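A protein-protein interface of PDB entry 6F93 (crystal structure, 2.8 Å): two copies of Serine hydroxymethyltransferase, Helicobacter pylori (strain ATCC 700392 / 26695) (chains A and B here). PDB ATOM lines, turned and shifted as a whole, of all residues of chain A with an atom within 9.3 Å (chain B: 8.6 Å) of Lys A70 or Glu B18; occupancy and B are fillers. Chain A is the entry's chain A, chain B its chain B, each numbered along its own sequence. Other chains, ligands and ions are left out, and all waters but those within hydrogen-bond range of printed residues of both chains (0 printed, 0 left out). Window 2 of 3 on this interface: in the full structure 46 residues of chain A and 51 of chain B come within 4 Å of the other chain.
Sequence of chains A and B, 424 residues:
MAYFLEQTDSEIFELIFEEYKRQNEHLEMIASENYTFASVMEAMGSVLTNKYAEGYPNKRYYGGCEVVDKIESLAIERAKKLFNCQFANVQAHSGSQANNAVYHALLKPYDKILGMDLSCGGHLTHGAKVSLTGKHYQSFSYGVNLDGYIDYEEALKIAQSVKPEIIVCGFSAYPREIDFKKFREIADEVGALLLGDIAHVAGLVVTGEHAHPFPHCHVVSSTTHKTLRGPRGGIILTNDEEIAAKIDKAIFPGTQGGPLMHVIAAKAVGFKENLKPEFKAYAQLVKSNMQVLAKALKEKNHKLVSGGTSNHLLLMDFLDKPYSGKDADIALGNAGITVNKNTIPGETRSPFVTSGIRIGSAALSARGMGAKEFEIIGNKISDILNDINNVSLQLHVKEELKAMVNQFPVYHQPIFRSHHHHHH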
ATOM      1  N   VAL A  47      -2.082  13.232  -3.851  1.00  0.00           N
ATOM      2  CA  VAL A  47      -2.287  12.356  -2.703  1.00  0.00           C
ATOM      3  C   VAL A  47      -1.240  12.624  -1.631  1.00  0.00           C
ATOM      4  O   VAL A  47      -1.265  12.008  -0.558  1.00  0.00           O
ATOM      5  CB  VAL A  47      -2.258  10.880  -3.126  1.00  0.00           C
ATOM      6  CG1 VAL A  47      -3.539  10.524  -3.841  1.00  0.00           C
ATOM      7  CG2 VAL A  47      -1.056  10.616  -4.018  1.00  0.00           C
ATOM      8  N   LEU A  48      -0.313  13.543  -1.912  1.00  0.00           N
ATOM      9  CA  LEU A  48       0.722  13.873  -0.939  1.00  0.00           C
ATOM     10  C   LEU A  48       0.153  14.503   0.323  1.00  0.00           C
ATOM     11  O   LEU A  48       0.840  14.524   1.352  1.00  0.00           O
ATOM     12  CB  LEU A  48       1.761  14.803  -1.565  1.00  0.00           C
ATOM     13  CG  LEU A  48       2.721  14.149  -2.559  1.00  0.00           C
ATOM     14  CD1 LEU A  48       3.788  15.132  -2.959  1.00  0.00           C
ATOM     15  CD2 LEU A  48       3.349  12.901  -1.965  1.00  0.00           C
ATOM     16  N   LYS A  51       0.386  11.912   3.362  1.00  0.00           N
ATOM     17  CA  LYS A  51       1.603  11.471   4.028  1.00  0.00           C
ATOM     18  C   LYS A  51       2.037  12.455   5.109  1.00  0.00           C
ATOM     19  O   LYS A  51       1.780  13.659   5.030  1.00  0.00           O
ATOM     20  CB  LYS A  51       2.732  11.290   3.015  1.00  0.00           C
ATOM     21  N   VAL A  67      15.419  13.524   9.962  1.00  0.00           N
ATOM     22  CA  VAL A  67      14.699  12.546   9.152  1.00  0.00           C
ATOM     23  C   VAL A  67      14.224  13.199   7.859  1.00  0.00           C
ATOM     24  O   VAL A  67      13.062  13.588   7.741  1.00  0.00           O
ATOM     25  CB  VAL A  67      13.523  11.935   9.930  1.00  0.00           C
ATOM     26  N   VAL A  68      15.127  13.303   6.888  1.00  0.00           N
ATOM     27  CA  VAL A  68      14.870  14.096   5.690  1.00  0.00           C
ATOM     28  C   VAL A  68      13.917  13.344   4.766  1.00  0.00           C
ATOM     29  O   VAL A  68      14.074  12.141   4.520  1.00  0.00           O
ATOM     30  CB  VAL A  68      16.191  14.461   4.983  1.00  0.00           C
ATOM     31  CG1 VAL A  68      17.191  15.021   5.986  1.00  0.00           C
ATOM     32  CG2 VAL A  68      16.804  13.267   4.264  1.00  0.00           C
ATOM     33  N   ASP A  69      12.898  14.050   4.284  1.00  0.00           N
ATOM     34  CA  ASP A  69      12.004  13.503   3.277  1.00  0.00           C
ATOM     35  C   ASP A  69      12.568  13.784   1.893  1.00  0.00           C
ATOM     36  O   ASP A  69      13.161  14.841   1.655  1.00  0.00           O
ATOM     37  CB  ASP A  69      10.607  14.110   3.408  1.00  0.00           C
ATOM     38  CG  ASP A  69       9.578  13.392   2.555  1.00  0.00           C
ATOM     39  OD1 ASP A  69       9.199  13.936   1.492  1.00  0.00           O
ATOM     40  OD2 ASP A  69       9.150  12.283   2.944  1.00  0.00           O
ATOM     41  N   LYS A  70      12.381  12.831   0.978  1.00  0.00           N
ATOM     42  CA  LYS A  70      12.895  12.999  -0.376  1.00  0.00           C
ATOM     43  C   LYS A  70      12.400  14.281  -1.032  1.00  0.00           C
ATOM     44  O   LYS A  70      13.104  14.858  -1.870  1.00  0.00           O
ATOM     45  CB  LYS A  70      12.509  11.796  -1.240  1.00  0.00           C
ATOM     46  CG  LYS A  70      13.295  10.526  -0.975  1.00  0.00           C
ATOM     47  CD  LYS A  70      13.191   9.576  -2.166  1.00  0.00           C
ATOM     48  CE  LYS A  70      13.766   8.202  -1.853  1.00  0.00           C
ATOM     49  NZ  LYS A  70      13.335   7.183  -2.855  1.00  0.00           N
ATOM     50  N   ILE A  71      11.206  14.745  -0.671  1.00  0.00           N
ATOM     51  CA  ILE A  71      10.602  15.857  -1.394  1.00  0.00           C
ATOM     52  C   ILE A  71      11.070  17.220  -0.884  1.00  0.00           C
ATOM     53  O   ILE A  71      11.213  18.158  -1.679  1.00  0.00           O
ATOM     54  CB  ILE A  71       9.072  15.731  -1.348  1.00  0.00           C
ATOM     55  CG1 ILE A  71       8.661  14.314  -1.735  1.00  0.00           C
ATOM     56  CG2 ILE A  71       8.434  16.734  -2.298  1.00  0.00           C
ATOM     57  CD1 ILE A  71       7.204  14.183  -2.162  1.00  0.00           C
ATOM     58  N   GLU A  72      11.328  17.363   0.416  1.00  0.00           N
ATOM     59  CA  GLU A  72      11.872  18.638   0.859  1.00  0.00           C
ATOM     60  C   GLU A  72      13.334  18.786   0.441  1.00  0.00           C
ATOM     61  O   GLU A  72      13.800  19.901   0.207  1.00  0.00           O
ATOM     62  CB  GLU A  72      11.701  18.807   2.372  1.00  0.00           C
ATOM     63  CG  GLU A  72      12.367  20.080   2.912  1.00  0.00           C
ATOM     64  CD  GLU A  72      11.918  20.473   4.316  1.00  0.00           C
ATOM     65  OE1 GLU A  72      12.097  21.659   4.664  1.00  0.00           O
ATOM     66  OE2 GLU A  72      11.393  19.598   5.034  1.00  0.00           O
ATOM     67  N   SER A  73      14.063  17.679   0.302  1.00  0.00           N
ATOM     68  CA  SER A  73      15.399  17.728  -0.278  1.00  0.00           C
ATOM     69  C   SER A  73      15.350  18.326  -1.675  1.00  0.00           C
ATOM     70  O   SER A  73      16.051  19.298  -1.976  1.00  0.00           O
ATOM     71  CB  SER A  73      15.998  16.323  -0.319  1.00  0.00           C
ATOM     72  OG  SER A  73      15.619  15.588   0.820  1.00  0.00           O
ATOM     73  N   LEU A  74      14.525  17.741  -2.549  1.00  0.00           N
ATOM     74  CA  LEU A  74      14.405  18.228  -3.917  1.00  0.00           C
ATOM     75  C   LEU A  74      13.961  19.685  -3.966  1.00  0.00           C
ATOM     76  O   LEU A  74      14.366  20.427  -4.872  1.00  0.00           O
ATOM     77  CB  LEU A  74      13.427  17.349  -4.685  1.00  0.00           C
ATOM     78  CG  LEU A  74      13.389  17.535  -6.196  1.00  0.00           C
ATOM     79  CD1 LEU A  74      14.782  17.436  -6.777  1.00  0.00           C
ATOM     80  CD2 LEU A  74      12.494  16.495  -6.806  1.00  0.00           C
ATOM     81  N   ALA A  75      13.130  20.113  -3.009  1.00  0.00           N
ATOM     82  CA  ALA A  75      12.752  21.520  -2.940  1.00  0.00           C
ATOM     83  C   ALA A  75      13.936  22.377  -2.517  1.00  0.00           C
ATOM     84  O   ALA A  75      14.202  23.425  -3.115  1.00  0.00           O
ATOM     85  CB  ALA A  75      11.579  21.700  -1.983  1.00  0.00           C
ATOM     86  N   ILE A  76      14.663  21.937  -1.486  1.00  0.00           N
ATOM     87  CA  ILE A  76      15.841  22.669  -1.027  1.00  0.00           C
ATOM     88  C   ILE A  76      16.932  22.642  -2.088  1.00  0.00           C
ATOM     89  O   ILE A  76      17.648  23.631  -2.284  1.00  0.00           O
ATOM     90  CB  ILE A  76      16.333  22.095   0.314  1.00  0.00           C
ATOM     91  CG1 ILE A  76      15.273  22.306   1.394  1.00  0.00           C
ATOM     92  CG2 ILE A  76      17.624  22.764   0.748  1.00  0.00           C
ATOM     93  CD1 ILE A  76      15.535  21.550   2.660  1.00  0.00           C
ATOM     94  N   GLU A  77      17.069  21.519  -2.796  1.00  0.00           N
ATOM     95  CA  GLU A  77      18.057  21.435  -3.867  1.00  0.00           C
ATOM     96  C   GLU A  77      17.784  22.478  -4.945  1.00  0.00           C
ATOM     97  O   GLU A  77      18.661  23.280  -5.293  1.00  0.00           O
ATOM     98  CB  GLU A  77      18.062  20.026  -4.467  1.00  0.00           C
ATOM     99  N   ARG A  78      16.559  22.486  -5.478  1.00  0.00           N
ATOM    100  CA  ARG A  78      16.208  23.450  -6.512  1.00  0.00           C
ATOM    101  C   ARG A  78      16.213  24.875  -5.969  1.00  0.00           C
ATOM    102  O   ARG A  78      16.601  25.810  -6.679  1.00  0.00           O
ATOM    103  CB  ARG A  78      14.848  23.092  -7.099  1.00  0.00           C
ATOM    104  CG  ARG A  78      14.836  21.736  -7.769  1.00  0.00           C
ATOM    105  CD  ARG A  78      13.443  21.352  -8.203  1.00  0.00           C
ATOM    106  NE  ARG A  78      13.420  20.071  -8.907  1.00  0.00           N
ATOM    107  CZ  ARG A  78      12.325  19.524  -9.431  1.00  0.00           C
ATOM    108  NH1 ARG A  78      12.398  18.355 -10.048  1.00  0.00           N
ATOM    109  NH2 ARG A  78      11.155  20.141  -9.333  1.00  0.00           N
ATOM    110  N   MET A 261       3.294  17.976   2.744  1.00  0.00           N
ATOM    111  CA  MET A 261       4.159  17.522   1.661  1.00  0.00           C
ATOM    112  C   MET A 261       3.677  18.019   0.307  1.00  0.00           C
ATOM    113  O   MET A 261       4.492  18.330  -0.571  1.00  0.00           O
ATOM    114  CB  MET A 261       4.232  16.000   1.692  1.00  0.00           C
ATOM    115  CG  MET A 261       5.074  15.474   2.845  1.00  0.00           C
ATOM    116  SD  MET A 261       6.809  15.893   2.610  1.00  0.00           S
ATOM    117  CE  MET A 261       7.085  17.010   3.971  1.00  0.00           C
ATOM    118  N   ILE A 264       4.954  21.439  -0.190  1.00  0.00           N
ATOM    119  CA  ILE A 264       6.395  21.451  -0.432  1.00  0.00           C
ATOM    120  C   ILE A 264       6.708  20.924  -1.829  1.00  0.00           C
ATOM    121  O   ILE A 264       7.526  21.504  -2.555  1.00  0.00           O
ATOM    122  CB  ILE A 264       7.128  20.654   0.665  1.00  0.00           C
ATOM    123  CG1 ILE A 264       7.035  21.394   2.000  1.00  0.00           C
ATOM    124  CG2 ILE A 264       8.590  20.427   0.298  1.00  0.00           C
ATOM    125  CD1 ILE A 264       7.668  20.665   3.160  1.00  0.00           C
ATOM    126  N   ALA A 265       6.060  19.824  -2.233  1.00  0.00           N
ATOM    127  CA  ALA A 265       6.211  19.356  -3.607  1.00  0.00           C
ATOM    128  C   ALA A 265       5.765  20.419  -4.595  1.00  0.00           C
ATOM    129  O   ALA A 265       6.382  20.591  -5.653  1.00  0.00           O
ATOM    130  CB  ALA A 265       5.426  18.069  -3.829  1.00  0.00           C
ATOM    131  N   ALA A 268       8.694  22.771  -4.906  1.00  0.00           N
ATOM    132  CA  ALA A 268       9.732  22.277  -5.803  1.00  0.00           C
ATOM    133  C   ALA A 268       9.286  22.360  -7.258  1.00  0.00           C
ATOM    134  O   ALA A 268      10.088  22.688  -8.140  1.00  0.00           O
ATOM    135  CB  ALA A 268      10.102  20.842  -5.434  1.00  0.00           C
ATOM    136  N   GLU B  11      10.411  14.216 -12.194  1.00  0.00           N
ATOM    137  CA  GLU B  11      11.015  13.846 -10.915  1.00  0.00           C
ATOM    138  C   GLU B  11      10.019  13.996  -9.771  1.00  0.00           C
ATOM    139  O   GLU B  11       9.902  13.110  -8.916  1.00  0.00           O
ATOM    140  CB  GLU B  11      12.263  14.687 -10.650  1.00  0.00           C
ATOM    141  CG  GLU B  11      13.081  14.190  -9.471  1.00  0.00           C
ATOM    142  CD  GLU B  11      14.433  14.881  -9.357  1.00  0.00           C
ATOM    143  OE1 GLU B  11      15.237  14.485  -8.479  1.00  0.00           O
ATOM    144  OE2 GLU B  11      14.691  15.821 -10.146  1.00  0.00           O
ATOM    145  N   ILE B  12       9.301  15.122  -9.729  1.00  0.00           N
ATOM    146  CA  ILE B  12       8.246  15.296  -8.734  1.00  0.00           C
ATOM    147  C   ILE B  12       7.136  14.275  -8.955  1.00  0.00           C
ATOM    148  O   ILE B  12       6.698  13.601  -8.014  1.00  0.00           O
ATOM    149  CB  ILE B  12       7.705  16.737  -8.762  1.00  0.00           C
ATOM    150  CG1 ILE B  12       8.616  17.665  -7.969  1.00  0.00           C
ATOM    151  CG2 ILE B  12       6.312  16.786  -8.175  1.00  0.00           C
ATOM    152  CD1 ILE B  12       8.662  17.325  -6.491  1.00  0.00           C
ATOM    153  N   PHE B  13       6.663  14.143 -10.204  1.00  0.00           N
ATOM    154  CA  PHE B  13       5.611  13.170 -10.486  1.00  0.00           C
ATOM    155  C   PHE B  13       6.037  11.771 -10.070  1.00  0.00           C
ATOM    156  O   PHE B  13       5.216  10.976  -9.593  1.00  0.00           O
ATOM    157  CB  PHE B  13       5.232  13.191 -11.967  1.00  0.00           C
ATOM    158  CG  PHE B  13       4.117  12.236 -12.318  1.00  0.00           C
ATOM    159  CD1 PHE B  13       4.378  10.904 -12.604  1.00  0.00           C
ATOM    160  CD2 PHE B  13       2.803  12.669 -12.348  1.00  0.00           C
ATOM    161  CE1 PHE B  13       3.354  10.031 -12.916  1.00  0.00           C
ATOM    162  CE2 PHE B  13       1.777  11.799 -12.656  1.00  0.00           C
ATOM    163  CZ  PHE B  13       2.055  10.480 -12.944  1.00  0.00           C
ATOM    164  N   GLU B  14       7.321  11.442 -10.250  1.00  0.00           N
ATOM    165  CA  GLU B  14       7.831  10.164  -9.766  1.00  0.00           C
ATOM    166  C   GLU B  14       7.581  10.004  -8.273  1.00  0.00           C
ATOM    167  O   GLU B  14       7.228   8.915  -7.808  1.00  0.00           O
ATOM    168  CB  GLU B  14       9.324  10.046 -10.077  1.00  0.00           C
ATOM    169  CG  GLU B  14       9.952   8.715  -9.685  1.00  0.00           C
ATOM    170  CD  GLU B  14      10.906   8.845  -8.515  1.00  0.00           C
ATOM    171  OE1 GLU B  14      10.855   7.987  -7.609  1.00  0.00           O
ATOM    172  OE2 GLU B  14      11.699   9.810  -8.497  1.00  0.00           O
ATOM    173  N   LEU B  15       7.740  11.086  -7.508  1.00  0.00           N
ATOM    174  CA  LEU B  15       7.517  11.026  -6.071  1.00  0.00           C
ATOM    175  C   LEU B  15       6.037  11.008  -5.717  1.00  0.00           C
ATOM    176  O   LEU B  15       5.656  10.397  -4.711  1.00  0.00           O
ATOM    177  CB  LEU B  15       8.197  12.216  -5.394  1.00  0.00           C
ATOM    178  CG  LEU B  15       9.705  12.327  -5.609  1.00  0.00           C
ATOM    179  CD1 LEU B  15      10.205  13.703  -5.184  1.00  0.00           C
ATOM    180  CD2 LEU B  15      10.431  11.210  -4.860  1.00  0.00           C
ATOM    181  N   ILE B  16       5.199  11.679  -6.510  1.00  0.00           N
ATOM    182  CA  ILE B  16       3.758  11.668  -6.267  1.00  0.00           C
ATOM    183  C   ILE B  16       3.187  10.283  -6.537  1.00  0.00           C
ATOM    184  O   ILE B  16       2.433   9.733  -5.726  1.00  0.00           O
ATOM    185  CB  ILE B  16       3.063  12.735  -7.130  1.00  0.00           C
ATOM    186  CG1 ILE B  16       3.442  14.140  -6.659  1.00  0.00           C
ATOM    187  CG2 ILE B  16       1.549  12.529  -7.132  1.00  0.00           C
ATOM    188  CD1 ILE B  16       3.059  15.220  -7.643  1.00  0.00           C
ATOM    189  N   PHE B  17       3.536   9.701  -7.684  1.00  0.00           N
ATOM    190  CA  PHE B  17       3.072   8.358  -8.015  1.00  0.00           C
ATOM    191  C   PHE B  17       3.672   7.308  -7.086  1.00  0.00           C
ATOM    192  O   PHE B  17       3.089   6.232  -6.909  1.00  0.00           O
ATOM    193  CB  PHE B  17       3.409   8.050  -9.475  1.00  0.00           C
ATOM    194  CG  PHE B  17       2.738   6.821 -10.013  1.00  0.00           C
ATOM    195  CD1 PHE B  17       1.363   6.780 -10.179  1.00  0.00           C
ATOM    196  CD2 PHE B  17       3.485   5.711 -10.369  1.00  0.00           C
ATOM    197  CE1 PHE B  17       0.746   5.650 -10.682  1.00  0.00           C
ATOM    198  CE2 PHE B  17       2.875   4.581 -10.874  1.00  0.00           C
ATOM    199  CZ  PHE B  17       1.504   4.551 -11.030  1.00  0.00           C
ATOM    200  N   GLU B  18       4.832   7.599  -6.490  1.00  0.00           N
ATOM    201  CA  GLU B  18       5.441   6.680  -5.532  1.00  0.00           C
ATOM    202  C   GLU B  18       4.654   6.644  -4.230  1.00  0.00           C
ATOM    203  O   GLU B  18       4.429   5.569  -3.662  1.00  0.00           O
ATOM    204  CB  GLU B  18       6.886   7.095  -5.269  1.00  0.00           C
ATOM    205  CG  GLU B  18       7.802   5.997  -4.773  1.00  0.00           C
ATOM    206  CD  GLU B  18       8.879   6.533  -3.841  1.00  0.00           C
ATOM    207  OE1 GLU B  18       8.551   6.858  -2.677  1.00  0.00           O
ATOM    208  OE2 GLU B  18      10.046   6.647  -4.278  1.00  0.00           O
ATOM    209  N   GLU B  19       4.236   7.814  -3.741  1.00  0.00           N
ATOM    210  CA  GLU B  19       3.426   7.871  -2.530  1.00  0.00           C
ATOM    211  C   GLU B  19       2.073   7.194  -2.730  1.00  0.00           C
ATOM    212  O   GLU B  19       1.597   6.472  -1.843  1.00  0.00           O
ATOM    213  CB  GLU B  19       3.247   9.327  -2.100  1.00  0.00           C
ATOM    214  CG  GLU B  19       2.017   9.585  -1.241  1.00  0.00           C
ATOM    215  CD  GLU B  19       2.236   9.211   0.210  1.00  0.00           C
ATOM    216  OE1 GLU B  19       1.246   9.185   0.972  1.00  0.00           O
ATOM    217  OE2 GLU B  19       3.402   8.948   0.589  1.00  0.00           O
ATOM    218  N   TYR B  20       1.448   7.406  -3.893  1.00  0.00           N
ATOM    219  CA  TYR B  20       0.149   6.800  -4.173  1.00  0.00           C
ATOM    220  C   TYR B  20       0.261   5.289  -4.306  1.00  0.00           C
ATOM    221  O   TYR B  20      -0.609   4.550  -3.836  1.00  0.00           O
ATOM    222  CB  TYR B  20      -0.447   7.415  -5.443  1.00  0.00           C
ATOM    223  CG  TYR B  20      -1.422   6.544  -6.213  1.00  0.00           C
ATOM    224  CD1 TYR B  20      -2.800   6.645  -5.989  1.00  0.00           C
ATOM    225  CD2 TYR B  20      -0.976   5.679  -7.217  1.00  0.00           C
ATOM    226  CE1 TYR B  20      -3.697   5.869  -6.699  1.00  0.00           C
ATOM    227  CE2 TYR B  20      -1.866   4.903  -7.935  1.00  0.00           C
ATOM    228  CZ  TYR B  20      -3.223   5.002  -7.675  1.00  0.00           C
ATOM    229  OH  TYR B  20      -4.104   4.231  -8.394  1.00  0.00           O
ATOM    230  N   LYS B  21       1.311   4.805  -4.967  1.00  0.00           N
ATOM    231  CA  LYS B  21       1.529   3.368  -5.051  1.00  0.00           C
ATOM    232  C   LYS B  21       1.775   2.768  -3.679  1.00  0.00           C
ATOM    233  O   LYS B  21       1.384   1.626  -3.426  1.00  0.00           O
ATOM    234  CB  LYS B  21       2.706   3.063  -5.977  1.00  0.00           C
ATOM    235  N   ARG B  22       2.408   3.524  -2.779  1.00  0.00           N
ATOM    236  CA  ARG B  22       2.718   2.992  -1.458  1.00  0.00           C
ATOM    237  C   ARG B  22       1.477   2.913  -0.579  1.00  0.00           C
ATOM    238  O   ARG B  22       1.336   1.974   0.213  1.00  0.00           O
ATOM    239  CB  ARG B  22       3.789   3.844  -0.780  1.00  0.00           C
ATOM    240  CG  ARG B  22       3.604   3.980   0.723  1.00  0.00           C
ATOM    241  CD  ARG B  22       4.433   5.107   1.300  1.00  0.00           C
ATOM    242  NE  ARG B  22       4.222   5.235   2.734  1.00  0.00           N
ATOM    243  CZ  ARG B  22       3.658   6.289   3.308  1.00  0.00           C
ATOM    244  NH1 ARG B  22       3.255   7.309   2.566  1.00  0.00           N
ATOM    245  NH2 ARG B  22       3.500   6.327   4.626  1.00  0.00           N
ATOM    246  N   GLN B  23       0.566   3.883  -0.705  1.00  0.00           N
ATOM    247  CA  GLN B  23      -0.651   3.864   0.102  1.00  0.00           C
ATOM    248  C   GLN B  23      -1.466   2.599  -0.127  1.00  0.00           C
ATOM    249  O   GLN B  23      -2.303   2.253   0.715  1.00  0.00           O
ATOM    250  CB  GLN B  23      -1.502   5.103  -0.188  1.00  0.00           C
ATOM    251  CG  GLN B  23      -1.059   6.356   0.563  1.00  0.00           C
ATOM    252  CD  GLN B  23      -1.608   7.651  -0.035  1.00  0.00           C
ATOM    253  OE1 GLN B  23      -2.627   7.656  -0.734  1.00  0.00           O
ATOM    254  NE2 GLN B  23      -0.930   8.758   0.248  1.00  0.00           N
ATOM    255  N   ASN B  24      -1.226   1.899  -1.234  1.00  0.00           N
ATOM    256  CA  ASN B  24      -1.897   0.645  -1.546  1.00  0.00           C
ATOM    257  C   ASN B  24      -0.966  -0.559  -1.426  1.00  0.00           C
ATOM    258  O   ASN B  24      -1.348  -1.667  -1.819  1.00  0.00           O
ATOM    259  CB  ASN B  24      -2.499   0.713  -2.956  1.00  0.00           C
ATOM    260  CG  ASN B  24      -3.328   1.983  -3.189  1.00  0.00           C
ATOM    261  OD1 ASN B  24      -2.811   3.097  -3.155  1.00  0.00           O
ATOM    262  ND2 ASN B  24      -4.624   1.808  -3.427  1.00  0.00           N
ATOM    263  N   GLU B  25       0.249  -0.365  -0.911  1.00  0.00           N
ATOM    264  CA  GLU B  25       1.241  -1.424  -0.777  1.00  0.00           C
ATOM    265  C   GLU B  25       1.422  -1.903   0.661  1.00  0.00           C
ATOM    266  O   GLU B  25       1.926  -3.015   0.872  1.00  0.00           O
ATOM    267  CB  GLU B  25       2.586  -0.947  -1.361  1.00  0.00           C
ATOM    268  CG  GLU B  25       3.858  -1.372  -0.611  1.00  0.00           C
ATOM    269  CD  GLU B  25       5.134  -0.880  -1.295  1.00  0.00           C
ATOM    270  OE1 GLU B  25       5.946  -1.739  -1.703  1.00  0.00           O
ATOM    271  OE2 GLU B  25       5.296   0.356  -1.407  1.00  0.00           O
ATOM    272  N   PRO B 414      -3.652   9.397  -9.164  1.00  0.00           N
ATOM    273  CA  PRO B 414      -2.699  10.059  -8.243  1.00  0.00           C
ATOM    274  C   PRO B 414      -3.019  11.528  -8.003  1.00  0.00           C
ATOM    275  O   PRO B 414      -2.764  12.034  -6.899  1.00  0.00           O
ATOM    276  CB  PRO B 414      -1.340   9.891  -8.952  1.00  0.00           C
ATOM    277  CG  PRO B 414      -1.678   9.668 -10.397  1.00  0.00           C
ATOM    278  CD  PRO B 414      -3.028   8.999 -10.429  1.00  0.00           C
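Val A47 touches Ile B16 (CG2 to O, 3.98 Å). CG2 of Val A47 touches CB of Tyr B20 (3.6 Å). CB of Glu B19 touches CD2 of Leu A48 (3.6 Å). CB of Lys A51 touches OE1 of Glu B19, at 3.3 Å. Ile A71 touches Leu B15. CD1 of Leu A74 touches OE1 of Glu B11 (3.4 Å). Ile B12 touches Leu A74. Leu A74 touches Leu B15 (CD2 to CD1, 3.96 Å). Arg A78 touches Ile B12. Ala A268 touches Ile B12 (CB to CD1, 3.9 Å).
O of Ala A268 lies within hydrogen-bond range of NH2 of Arg A78. The backbone carbonyl oxygen (O) of Tyr B20 lies close to the side-chain amide oxygen (OD1) of Asn B24 (2.7 Å). OE2 of Glu B19 is in salt-bridge range of NH1 of Arg B22, at 2.6 Å. The side-chain carboxylate (OD1) of Asp A69 lies close to the backbone NH (N) of Ile A71, 3.1 Å away.
Printed residues of chain B within 4 Å of Lys A70: Glu B18 (3.6 Å). Glu B18 touches one residue of chain A. No residue of chain B comes within 4 Å of Asp A69. No residue of chain A comes within 4 Å of Lys B21. Printed residues of chain A within 4 Å of Ile B16: Val A47 (3.98 Å) and Leu A48 (3.8 Å). Of the printed residues of chain A, Ile B12 touches Leu A74 (3.9 Å), Arg A78 (3.8 Å) and Ala A268 (3.9 Å). Of the printed residues of chain B, Val A47 touches Ile B16, Tyr B20, Gln B23 and Pro B414. Printed residues of chain A within 4 Å of Pro B414: Val A47. Of the printed residues of chain B, Arg A78 touches Glu B11 and Ile B12. Ile A264 touches none of the printed residues of chain B. The nearest printed residue of chain A that does not touch Gln B23 is Lys A51 (4.6 Å).
Hydrophobic or aromatic side chains of chain B that line the printed part of chain A: Ile B12, Leu B15, Ile B16 and Tyr B20. Of the 19 printed residues of chain A, 8 touch a printed residue of chain B. Printed residues of chain A that touch a printed residue of chain B: Val A47, Leu A48, Lys A51, Lys A70, Ile A71, Leu A74, Arg A78 and Ala A268. Among the printed residues, Asp or Glu carboxylates within 4 Å of a Lys or Arg side-chain nitrogen of the other chain: Lys A70 with Glu B18 (3.6 Å) and Arg A78 with Glu B11 (3.4 Å).
The side-chain carboxylate (OE2) of Glu B11 is in salt-bridge range of the guanidinium group (NH1) of Arg A78, at 3.4 Å. The backbone carbonyl oxygen of Val A47 sits at hydrogen-bond distance from the side-chain amide nitrogen of Gln B23 (3.4 Å). The backbone NH (N) of Val A47 is in hydrogen-bond range of the backbone carbonyl oxygen (O) of Pro B414 (3.3 Å). The side-chain amino group of Lys A70 is in salt-bridge range of the side-chain carboxylate of Glu B18, at 3.6 Å.
No position is printed for both chains. Of the 15 pairs that touch across the chains among the printed residues, none has its exchanged pair printed and touching as well.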
